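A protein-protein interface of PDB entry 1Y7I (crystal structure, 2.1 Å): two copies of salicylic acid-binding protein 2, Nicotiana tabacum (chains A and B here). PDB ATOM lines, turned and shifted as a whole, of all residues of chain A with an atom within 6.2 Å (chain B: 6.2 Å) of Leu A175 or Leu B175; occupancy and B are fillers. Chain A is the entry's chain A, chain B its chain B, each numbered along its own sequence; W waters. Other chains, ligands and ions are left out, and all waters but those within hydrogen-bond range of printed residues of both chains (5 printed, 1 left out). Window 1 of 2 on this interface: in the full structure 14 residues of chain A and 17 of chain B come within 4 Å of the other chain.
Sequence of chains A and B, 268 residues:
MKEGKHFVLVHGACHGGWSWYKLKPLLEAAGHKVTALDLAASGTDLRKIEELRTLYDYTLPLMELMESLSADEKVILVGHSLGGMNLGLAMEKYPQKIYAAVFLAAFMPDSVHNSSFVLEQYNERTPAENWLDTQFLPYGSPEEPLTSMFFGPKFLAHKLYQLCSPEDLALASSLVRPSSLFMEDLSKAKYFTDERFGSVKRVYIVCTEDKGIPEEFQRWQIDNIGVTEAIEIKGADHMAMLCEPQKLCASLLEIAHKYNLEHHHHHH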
ATOM      1  N   CYS A  14      -7.189 -20.601   4.618  1.00  0.00           N
ATOM      2  CA  CYS A  14      -7.065 -20.009   3.289  1.00  0.00           C
ATOM      3  C   CYS A  14      -8.388 -19.850   2.557  1.00  0.00           C
ATOM      4  O   CYS A  14      -8.428 -19.343   1.438  1.00  0.00           O
ATOM      5  CB  CYS A  14      -6.089 -20.831   2.441  1.00  0.00           C
ATOM      6  SG  CYS A  14      -4.459 -21.079   3.236  1.00  0.00           S
ATOM      7  N   HIS A  15      -9.474 -20.272   3.193  1.00  0.00           N
ATOM      8  CA  HIS A  15     -10.793 -20.167   2.588  1.00  0.00           C
ATOM      9  C   HIS A  15     -11.638 -19.080   3.246  1.00  0.00           C
ATOM     10  O   HIS A  15     -11.136 -18.303   4.055  1.00  0.00           O
ATOM     11  CB  HIS A  15     -11.491 -21.529   2.656  1.00  0.00           C
ATOM     12  CG  HIS A  15     -10.985 -22.499   1.635  1.00  0.00           C
ATOM     13  ND1 HIS A  15      -9.696 -22.988   1.649  1.00  0.00           N
ATOM     14  CD2 HIS A  15     -11.568 -23.002   0.521  1.00  0.00           C
ATOM     15  CE1 HIS A  15      -9.507 -23.752   0.585  1.00  0.00           C
ATOM     16  NE2 HIS A  15     -10.627 -23.777  -0.114  1.00  0.00           N
ATOM     17  N   TRP A  18     -17.368 -17.858   1.431  1.00  0.00           N
ATOM     18  CA  TRP A  18     -17.762 -18.171   0.056  1.00  0.00           C
ATOM     19  C   TRP A  18     -17.693 -19.680  -0.216  1.00  0.00           C
ATOM     20  O   TRP A  18     -18.441 -20.193  -1.034  1.00  0.00           O
ATOM     21  CB  TRP A  18     -16.856 -17.428  -0.945  1.00  0.00           C
ATOM     22  CG  TRP A  18     -15.393 -17.723  -0.766  1.00  0.00           C
ATOM     23  CD1 TRP A  18     -14.496 -17.015  -0.012  1.00  0.00           C
ATOM     24  CD2 TRP A  18     -14.666 -18.834  -1.312  1.00  0.00           C
ATOM     25  NE1 TRP A  18     -13.260 -17.621  -0.053  1.00  0.00           N
ATOM     26  CE2 TRP A  18     -13.339 -18.738  -0.843  1.00  0.00           C
ATOM     27  CE3 TRP A  18     -15.011 -19.902  -2.149  1.00  0.00           C
ATOM     28  CZ2 TRP A  18     -12.352 -19.670  -1.185  1.00  0.00           C
ATOM     29  CZ3 TRP A  18     -14.035 -20.831  -2.491  1.00  0.00           C
ATOM     30  CH2 TRP A  18     -12.720 -20.709  -2.010  1.00  0.00           C
ATOM     31  N   ASP A  38     -16.796 -14.862   7.421  1.00  0.00           N
ATOM     32  CA  ASP A  38     -15.391 -14.825   7.062  1.00  0.00           C
ATOM     33  C   ASP A  38     -14.674 -14.621   8.385  1.00  0.00           C
ATOM     34  O   ASP A  38     -15.071 -13.765   9.175  1.00  0.00           O
ATOM     35  CB  ASP A  38     -15.090 -13.621   6.176  1.00  0.00           C
ATOM     36  CG  ASP A  38     -15.593 -13.789   4.766  1.00  0.00           C
ATOM     37  OD1 ASP A  38     -15.729 -12.760   4.075  1.00  0.00           O
ATOM     38  OD2 ASP A  38     -15.841 -14.941   4.348  1.00  0.00           O
ATOM     39  N   GLY A  43     -11.628 -14.499   3.287  1.00  0.00           N
ATOM     40  CA  GLY A  43     -12.643 -14.055   2.351  1.00  0.00           C
ATOM     41  C   GLY A  43     -12.425 -12.596   1.997  1.00  0.00           C
ATOM     42  O   GLY A  43     -11.357 -12.210   1.510  1.00  0.00           O
ATOM     43  N   THR A  44     -13.436 -11.778   2.262  1.00  0.00           N
ATOM     44  CA  THR A  44     -13.361 -10.355   1.972  1.00  0.00           C
ATOM     45  C   THR A  44     -13.037  -9.502   3.206  1.00  0.00           C
ATOM     46  O   THR A  44     -13.118  -8.274   3.157  1.00  0.00           O
ATOM     47  CB  THR A  44     -14.678  -9.864   1.328  1.00  0.00           C
ATOM     48  OG1 THR A  44     -15.793 -10.312   2.111  1.00  0.00           O
ATOM     49  CG2 THR A  44     -14.813 -10.421  -0.087  1.00  0.00           C
ATOM     50  N   ALA A 170     -10.706 -23.215  -9.976  1.00  0.00           N
ATOM     51  CA  ALA A 170     -10.412 -21.869 -10.428  1.00  0.00           C
ATOM     52  C   ALA A 170     -10.980 -20.837  -9.449  1.00  0.00           C
ATOM     53  O   ALA A 170     -10.395 -19.772  -9.263  1.00  0.00           O
ATOM     54  CB  ALA A 170     -10.979 -21.640 -11.835  1.00  0.00           C
ATOM     55  N   LEU A 171     -12.119 -21.144  -8.829  1.00  0.00           N
ATOM     56  CA  LEU A 171     -12.707 -20.216  -7.869  1.00  0.00           C
ATOM     57  C   LEU A 171     -11.770 -20.101  -6.663  1.00  0.00           C
ATOM     58  O   LEU A 171     -11.461 -18.996  -6.201  1.00  0.00           O
ATOM     59  CB  LEU A 171     -14.085 -20.701  -7.404  1.00  0.00           C
ATOM     60  CG  LEU A 171     -14.825 -19.821  -6.376  1.00  0.00           C
ATOM     61  CD1 LEU A 171     -15.071 -18.446  -6.945  1.00  0.00           C
ATOM     62  CD2 LEU A 171     -16.140 -20.485  -5.990  1.00  0.00           C
ATOM     63  N   ALA A 172     -11.315 -21.248  -6.167  1.00  0.00           N
ATOM     64  CA  ALA A 172     -10.412 -21.290  -5.014  1.00  0.00           C
ATOM     65  C   ALA A 172      -9.099 -20.553  -5.277  1.00  0.00           C
ATOM     66  O   ALA A 172      -8.626 -19.782  -4.441  1.00  0.00           O
ATOM     67  CB  ALA A 172     -10.113 -22.735  -4.632  1.00  0.00           C
ATOM     68  N   SER A 173      -8.509 -20.800  -6.439  1.00  0.00           N
ATOM     69  CA  SER A 173      -7.247 -20.165  -6.786  1.00  0.00           C
ATOM     70  C   SER A 173      -7.414 -18.654  -6.860  1.00  0.00           C
ATOM     71  O   SER A 173      -6.455 -17.901  -6.707  1.00  0.00           O
ATOM     72  CB  SER A 173      -6.730 -20.712  -8.121  1.00  0.00           C
ATOM     73  OG  SER A 173      -6.414 -22.095  -8.000  1.00  0.00           O
ATOM     74  N   SER A 174      -8.640 -18.209  -7.088  1.00  0.00           N
ATOM     75  CA  SER A 174      -8.899 -16.786  -7.166  1.00  0.00           C
ATOM     76  C   SER A 174      -9.283 -16.155  -5.832  1.00  0.00           C
ATOM     77  O   SER A 174      -9.300 -14.930  -5.713  1.00  0.00           O
ATOM     78  CB  SER A 174     -10.006 -16.507  -8.173  1.00  0.00           C
ATOM     79  OG  SER A 174     -10.467 -15.176  -8.026  1.00  0.00           O
ATOM     80  N   LEU A 175      -9.584 -16.967  -4.825  1.00  0.00           N
ATOM     81  CA  LEU A 175      -9.990 -16.404  -3.543  1.00  0.00           C
ATOM     82  C   LEU A 175      -9.149 -16.778  -2.336  1.00  0.00           C
ATOM     83  O   LEU A 175      -9.237 -16.117  -1.303  1.00  0.00           O
ATOM     84  CB  LEU A 175     -11.439 -16.780  -3.251  1.00  0.00           C
ATOM     85  CG  LEU A 175     -12.505 -16.205  -4.179  1.00  0.00           C
ATOM     86  CD1 LEU A 175     -13.820 -16.897  -3.885  1.00  0.00           C
ATOM     87  CD2 LEU A 175     -12.643 -14.680  -3.950  1.00  0.00           C
ATOM     88  N   VAL A 176      -8.343 -17.828  -2.445  1.00  0.00           N
ATOM     89  CA  VAL A 176      -7.544 -18.230  -1.300  1.00  0.00           C
ATOM     90  C   VAL A 176      -6.586 -17.133  -0.844  1.00  0.00           C
ATOM     91  O   VAL A 176      -6.055 -16.369  -1.653  1.00  0.00           O
ATOM     92  CB  VAL A 176      -6.755 -19.537  -1.572  1.00  0.00           C
ATOM     93  CG1 VAL A 176      -7.722 -20.714  -1.641  1.00  0.00           C
ATOM     94  CG2 VAL A 176      -5.950 -19.417  -2.858  1.00  0.00           C
ATOM     95  N   ARG A 177      -6.401 -17.059   0.467  1.00  0.00           N
ATOM     96  CA  ARG A 177      -5.525 -16.074   1.076  1.00  0.00           C
ATOM     97  C   ARG A 177      -4.694 -16.790   2.135  1.00  0.00           C
ATOM     98  O   ARG A 177      -5.094 -17.831   2.650  1.00  0.00           O
ATOM     99  CB  ARG A 177      -6.355 -14.957   1.725  1.00  0.00           C
ATOM    100  CG  ARG A 177      -7.185 -14.140   0.743  1.00  0.00           C
ATOM    101  CD  ARG A 177      -8.083 -13.138   1.471  1.00  0.00           C
ATOM    102  NE  ARG A 177      -7.339 -12.267   2.376  1.00  0.00           N
ATOM    103  CZ  ARG A 177      -7.906 -11.413   3.225  1.00  0.00           C
ATOM    104  NH1 ARG A 177      -9.227 -11.313   3.285  1.00  0.00           N
ATOM    105  NH2 ARG A 177      -7.151 -10.665   4.020  1.00  0.00           N
ATOM    106  N   CYS B  14     -18.577  -4.094  -7.892  1.00  0.00           N
ATOM    107  CA  CYS B  14     -18.894  -4.894  -6.733  1.00  0.00           C
ATOM    108  C   CYS B  14     -18.466  -6.348  -6.862  1.00  0.00           C
ATOM    109  O   CYS B  14     -18.651  -7.139  -5.936  1.00  0.00           O
ATOM    110  CB  CYS B  14     -20.395  -4.791  -6.435  1.00  0.00           C
ATOM    111  SG  CYS B  14     -20.976  -3.060  -6.250  1.00  0.00           S
ATOM    112  N   HIS B  15     -17.886  -6.711  -8.001  1.00  0.00           N
ATOM    113  CA  HIS B  15     -17.430  -8.082  -8.187  1.00  0.00           C
ATOM    114  C   HIS B  15     -15.901  -8.158  -8.226  1.00  0.00           C
ATOM    115  O   HIS B  15     -15.222  -7.169  -7.967  1.00  0.00           O
ATOM    116  CB  HIS B  15     -18.041  -8.677  -9.462  1.00  0.00           C
ATOM    117  CG  HIS B  15     -19.493  -9.020  -9.328  1.00  0.00           C
ATOM    118  ND1 HIS B  15     -20.470  -8.065  -9.154  1.00  0.00           N
ATOM    119  CD2 HIS B  15     -20.133 -10.217  -9.324  1.00  0.00           C
ATOM    120  CE1 HIS B  15     -21.649  -8.655  -9.047  1.00  0.00           C
ATOM    121  NE2 HIS B  15     -21.472  -9.961  -9.146  1.00  0.00           N
ATOM    122  N   TRP B  18     -12.927 -13.502  -9.224  1.00  0.00           N
ATOM    123  CA  TRP B  18     -13.654 -14.733  -8.931  1.00  0.00           C
ATOM    124  C   TRP B  18     -14.884 -14.902  -9.812  1.00  0.00           C
ATOM    125  O   TRP B  18     -15.376 -16.013 -10.001  1.00  0.00           O
ATOM    126  CB  TRP B  18     -14.104 -14.751  -7.463  1.00  0.00           C
ATOM    127  CG  TRP B  18     -15.015 -13.597  -7.081  1.00  0.00           C
ATOM    128  CD1 TRP B  18     -14.637 -12.405  -6.538  1.00  0.00           C
ATOM    129  CD2 TRP B  18     -16.443 -13.539  -7.217  1.00  0.00           C
ATOM    130  NE1 TRP B  18     -15.737 -11.604  -6.322  1.00  0.00           N
ATOM    131  CE2 TRP B  18     -16.858 -12.277  -6.732  1.00  0.00           C
ATOM    132  CE3 TRP B  18     -17.413 -14.428  -7.703  1.00  0.00           C
ATOM    133  CZ2 TRP B  18     -18.201 -11.881  -6.719  1.00  0.00           C
ATOM    134  CZ3 TRP B  18     -18.750 -14.035  -7.690  1.00  0.00           C
ATOM    135  CH2 TRP B  18     -19.130 -12.767  -7.198  1.00  0.00           C
ATOM    136  N   ASP B  38      -8.087  -8.723 -10.181  1.00  0.00           N
ATOM    137  CA  ASP B  38      -8.898  -8.174  -9.108  1.00  0.00           C
ATOM    138  C   ASP B  38      -8.584  -6.683  -9.231  1.00  0.00           C
ATOM    139  O   ASP B  38      -7.416  -6.297  -9.209  1.00  0.00           O
ATOM    140  CB  ASP B  38      -8.431  -8.669  -7.740  1.00  0.00           C
ATOM    141  CG  ASP B  38      -9.348  -9.718  -7.141  1.00  0.00           C
ATOM    142  OD1 ASP B  38      -9.031 -10.230  -6.043  1.00  0.00           O
ATOM    143  OD2 ASP B  38     -10.388 -10.037  -7.752  1.00  0.00           O
ATOM    144  N   GLY B  43     -12.709  -8.087  -5.021  1.00  0.00           N
ATOM    145  CA  GLY B  43     -12.277  -9.440  -4.709  1.00  0.00           C
ATOM    146  C   GLY B  43     -11.593  -9.529  -3.355  1.00  0.00           C
ATOM    147  O   GLY B  43     -12.211  -9.244  -2.332  1.00  0.00           O
ATOM    148  N   THR B  44     -10.326  -9.930  -3.333  1.00  0.00           N
ATOM    149  CA  THR B  44      -9.602 -10.018  -2.067  1.00  0.00           C
ATOM    150  C   THR B  44      -8.547  -8.920  -1.955  1.00  0.00           C
ATOM    151  O   THR B  44      -7.676  -8.989  -1.096  1.00  0.00           O
ATOM    152  CB  THR B  44      -8.901 -11.392  -1.873  1.00  0.00           C
ATOM    153  OG1 THR B  44      -8.081 -11.679  -3.013  1.00  0.00           O
ATOM    154  CG2 THR B  44      -9.926 -12.502  -1.665  1.00  0.00           C
ATOM    155  N   ALA B 170     -25.728 -17.085  -3.784  1.00  0.00           N
ATOM    156  CA  ALA B 170     -25.078 -17.212  -2.482  1.00  0.00           C
ATOM    157  C   ALA B 170     -23.601 -16.823  -2.602  1.00  0.00           C
ATOM    158  O   ALA B 170     -23.061 -16.145  -1.736  1.00  0.00           O
ATOM    159  CB  ALA B 170     -25.207 -18.634  -1.964  1.00  0.00           C
ATOM    160  N   LEU B 171     -22.947 -17.245  -3.679  1.00  0.00           N
ATOM    161  CA  LEU B 171     -21.535 -16.911  -3.866  1.00  0.00           C
ATOM    162  C   LEU B 171     -21.345 -15.395  -3.910  1.00  0.00           C
ATOM    163  O   LEU B 171     -20.522 -14.844  -3.192  1.00  0.00           O
ATOM    164  CB  LEU B 171     -21.002 -17.539  -5.157  1.00  0.00           C
ATOM    165  CG  LEU B 171     -19.505 -17.332  -5.446  1.00  0.00           C
ATOM    166  CD1 LEU B 171     -18.654 -17.863  -4.291  1.00  0.00           C
ATOM    167  CD2 LEU B 171     -19.153 -18.051  -6.738  1.00  0.00           C
ATOM    168  N   ALA B 172     -22.129 -14.725  -4.748  1.00  0.00           N
ATOM    169  CA  ALA B 172     -22.050 -13.278  -4.895  1.00  0.00           C
ATOM    170  C   ALA B 172     -22.330 -12.551  -3.587  1.00  0.00           C
ATOM    171  O   ALA B 172     -21.687 -11.551  -3.269  1.00  0.00           O
ATOM    172  CB  ALA B 172     -23.036 -12.808  -5.972  1.00  0.00           C
ATOM    173  N   SER B 173     -23.302 -13.048  -2.833  1.00  0.00           N
ATOM    174  CA  SER B 173     -23.671 -12.426  -1.570  1.00  0.00           C
ATOM    175  C   SER B 173     -22.527 -12.458  -0.548  1.00  0.00           C
ATOM    176  O   SER B 173     -22.423 -11.573   0.303  1.00  0.00           O
ATOM    177  CB  SER B 173     -24.927 -13.111  -1.014  1.00  0.00           C
ATOM    178  OG  SER B 173     -25.278 -12.609   0.264  1.00  0.00           O
ATOM    179  N   SER B 174     -21.664 -13.463  -0.627  1.00  0.00           N
ATOM    180  CA  SER B 174     -20.548 -13.546   0.309  1.00  0.00           C
ATOM    181  C   SER B 174     -19.301 -12.842  -0.217  1.00  0.00           C
ATOM    182  O   SER B 174     -18.300 -12.742   0.494  1.00  0.00           O
ATOM    183  CB  SER B 174     -20.189 -14.999   0.581  1.00  0.00           C
ATOM    184  OG  SER B 174     -19.650 -15.575  -0.594  1.00  0.00           O
ATOM    185  N   LEU B 175     -19.345 -12.356  -1.453  1.00  0.00           N
ATOM    186  CA  LEU B 175     -18.174 -11.702  -2.025  1.00  0.00           C
ATOM    187  C   LEU B 175     -18.340 -10.258  -2.501  1.00  0.00           C
ATOM    188  O   LEU B 175     -17.352  -9.524  -2.566  1.00  0.00           O
ATOM    189  CB  LEU B 175     -17.625 -12.554  -3.179  1.00  0.00           C
ATOM    190  CG  LEU B 175     -17.155 -13.962  -2.800  1.00  0.00           C
ATOM    191  CD1 LEU B 175     -16.890 -14.813  -4.047  1.00  0.00           C
ATOM    192  CD2 LEU B 175     -15.886 -13.846  -1.961  1.00  0.00           C
ATOM    193  N   VAL B 176     -19.560  -9.836  -2.840  1.00  0.00           N
ATOM    194  CA  VAL B 176     -19.740  -8.463  -3.324  1.00  0.00           C
ATOM    195  C   VAL B 176     -19.264  -7.399  -2.341  1.00  0.00           C
ATOM    196  O   VAL B 176     -19.442  -7.517  -1.129  1.00  0.00           O
ATOM    197  CB  VAL B 176     -21.216  -8.154  -3.743  1.00  0.00           C
ATOM    198  CG1 VAL B 176     -21.570  -8.961  -4.987  1.00  0.00           C
ATOM    199  CG2 VAL B 176     -22.197  -8.462  -2.603  1.00  0.00           C
ATOM    200  N   ARG B 177     -18.619  -6.373  -2.884  1.00  0.00           N
ATOM    201  CA  ARG B 177     -18.104  -5.280  -2.081  1.00  0.00           C
ATOM    202  C   ARG B 177     -18.493  -3.979  -2.750  1.00  0.00           C
ATOM    203  O   ARG B 177     -18.789  -3.951  -3.942  1.00  0.00           O
ATOM    204  CB  ARG B 177     -16.579  -5.360  -1.968  1.00  0.00           C
ATOM    205  CG  ARG B 177     -16.056  -6.590  -1.234  1.00  0.00           C
ATOM    206  CD  ARG B 177     -14.539  -6.701  -1.373  1.00  0.00           C
ATOM    207  NE  ARG B 177     -13.851  -5.510  -0.872  1.00  0.00           N
ATOM    208  CZ  ARG B 177     -12.545  -5.291  -0.983  1.00  0.00           C
ATOM    209  NH1 ARG B 177     -11.766  -6.183  -1.583  1.00  0.00           N
ATOM    210  NH2 ARG B 177     -12.020  -4.175  -0.498  1.00  0.00           N
HETATM  211  O   HOH W   1     -16.100 -14.912   1.745  1.00  0.00           O
HETATM  212  O   HOH W   2     -18.400  -9.702   0.979  1.00  0.00           O
HETATM  213  O   HOH W   3     -18.240 -13.039   3.508  1.00  0.00           O
HETATM  214  O   HOH W   4      -8.197 -12.825  -6.648  1.00  0.00           O
HETATM  215  O   HOH W   5     -11.549 -12.260  -6.825  1.00  0.00           O
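The backbone NH (N) of Trp B18 is in hydrogen-bond range of the side-chain hydroxyl (OG) of Ser A174, at 3.2 Å.
N of Thr B44 is in hydrogen-bond range of OD1 of Asp B38. The backbone NH (N) of Arg A177 sits at hydrogen-bond distance from the backbone carbonyl oxygen (O) of Cys A14 (3.2 Å). The side-chain carboxylate (OD1) of Asp A38 sits at hydrogen-bond distance from the backbone NH (N) of Thr A44, 3.1 Å away. The guanidinium group (NH1) of Arg B177 sits at hydrogen-bond distance from the backbone carbonyl oxygen (O) of Gly B43, at 3.2 Å. The guanidinium group (NH1) of Arg A177 sits at hydrogen-bond distance from the backbone carbonyl oxygen (O) of Gly A43. The backbone carbonyl oxygen (O) of Leu B171 is in hydrogen-bond range of the side-chain hydroxyl (OG) of Ser B174 (2.8 Å).
Among the printed residues, merely in contact across the chains: Trp A18 with Ser B174 (3.3 Å), Gly A43 with Thr B44 (3.5 Å), Thr A44 with Gly B43 (3.6 Å), Thr A44 with Leu B175 (3.7 Å), Arg A177 with Thr B44 (3.7 Å), Leu A175 with Thr B44 (3.7 Å), Leu A175 with Leu B175 (3.7 Å), Leu A175 with Trp B18 (3.8 Å), Trp A18 with Leu B171 (3.8 Å), Trp A18 with Leu B175 (3.8 Å), Thr A44 with Ser B174 (3.8 Å), Leu A171 with Trp B18 (3.9 Å), Leu A171 with Leu B171 (3.9 Å) and Thr A44 with Arg B177 (3.9 Å).
Leu A175 touches just these residues of chain B: Trp B18 (3.8 Å), Thr B44 (3.7 Å) and Leu B175 (3.7 Å). Of chain A, only Trp A18 (3.8 Å), Thr A44 (3.7 Å) and Leu A175 (3.7 Å) come within 4 Å of Leu B175. Printed residues of chain B within 4 Å of Gly A43: Thr B44. Of the printed residues of chain A, Thr B44 touches Gly A43, Leu A175 and Arg A177. Of the printed residues of chain A, Gly B43 touches Thr A44. Of the printed residues of chain B, Ser A174 touches Trp B18. The nearest residue of chain A that does not touch Leu B175 is Leu A171 (5.0 Å).
Hydrophobic or aromatic side chains of chain A that line the printed part of chain B: Trp A18, Leu A171 and Leu A175. Among the printed residues, 15 pairs touch across the chains. Among the printed residues, no Asp or Glu carboxylate lies within 4 Å of a Lys or Arg side-chain nitrogen of the other chain.
Trp A18 touches Leu B171, and with the chains exchanged Leu A171 touches Trp B18. Trp A18 touches Ser B174, and with the chains exchanged Ser A174 touches Trp B18. Gly A43 touches Thr B44, and with the chains exchanged Thr A44 touches Gly B43. Thr A44 touches Leu B175, and with the chains exchanged Leu A175 touches Thr B44. Of the 15 pairs that touch across the chains among the printed residues, 14 have their exchanged pair printed and touching as well.
Water W4 lies within hydrogen-bond range of the backbone carbonyl oxygen of Ser A174 (2.6 Å) and the side-chain carboxylate of Asp B38 (2.8 Å). Water W3 bridges the side-chain carboxylate of Asp A38 (2.6 Å) and the backbone carbonyl oxygen of Ser B174 (3.0 Å). Water W1 lies within hydrogen-bond range of OD2 of Asp A38 (2.6 Å), N of Trp A18 (3.2 Å) and O of Ser B174 (3.3 Å). Water W5 lies within hydrogen-bond range of the side-chain carboxylate (OD2) of Asp B38 (2.7 Å), the backbone NH (N) of Trp B18 (3.0 Å) and the side-chain hydroxyl (OG) of Ser A174 (3.3 Å). Water W2 lies within hydrogen-bond range of the side-chain hydroxyl of Thr A44 (2.9 Å), the backbone carbonyl oxygen of Ser B174 (3.1 Å) and the backbone carbonyl oxygen of Val B176 (3.2 Å).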
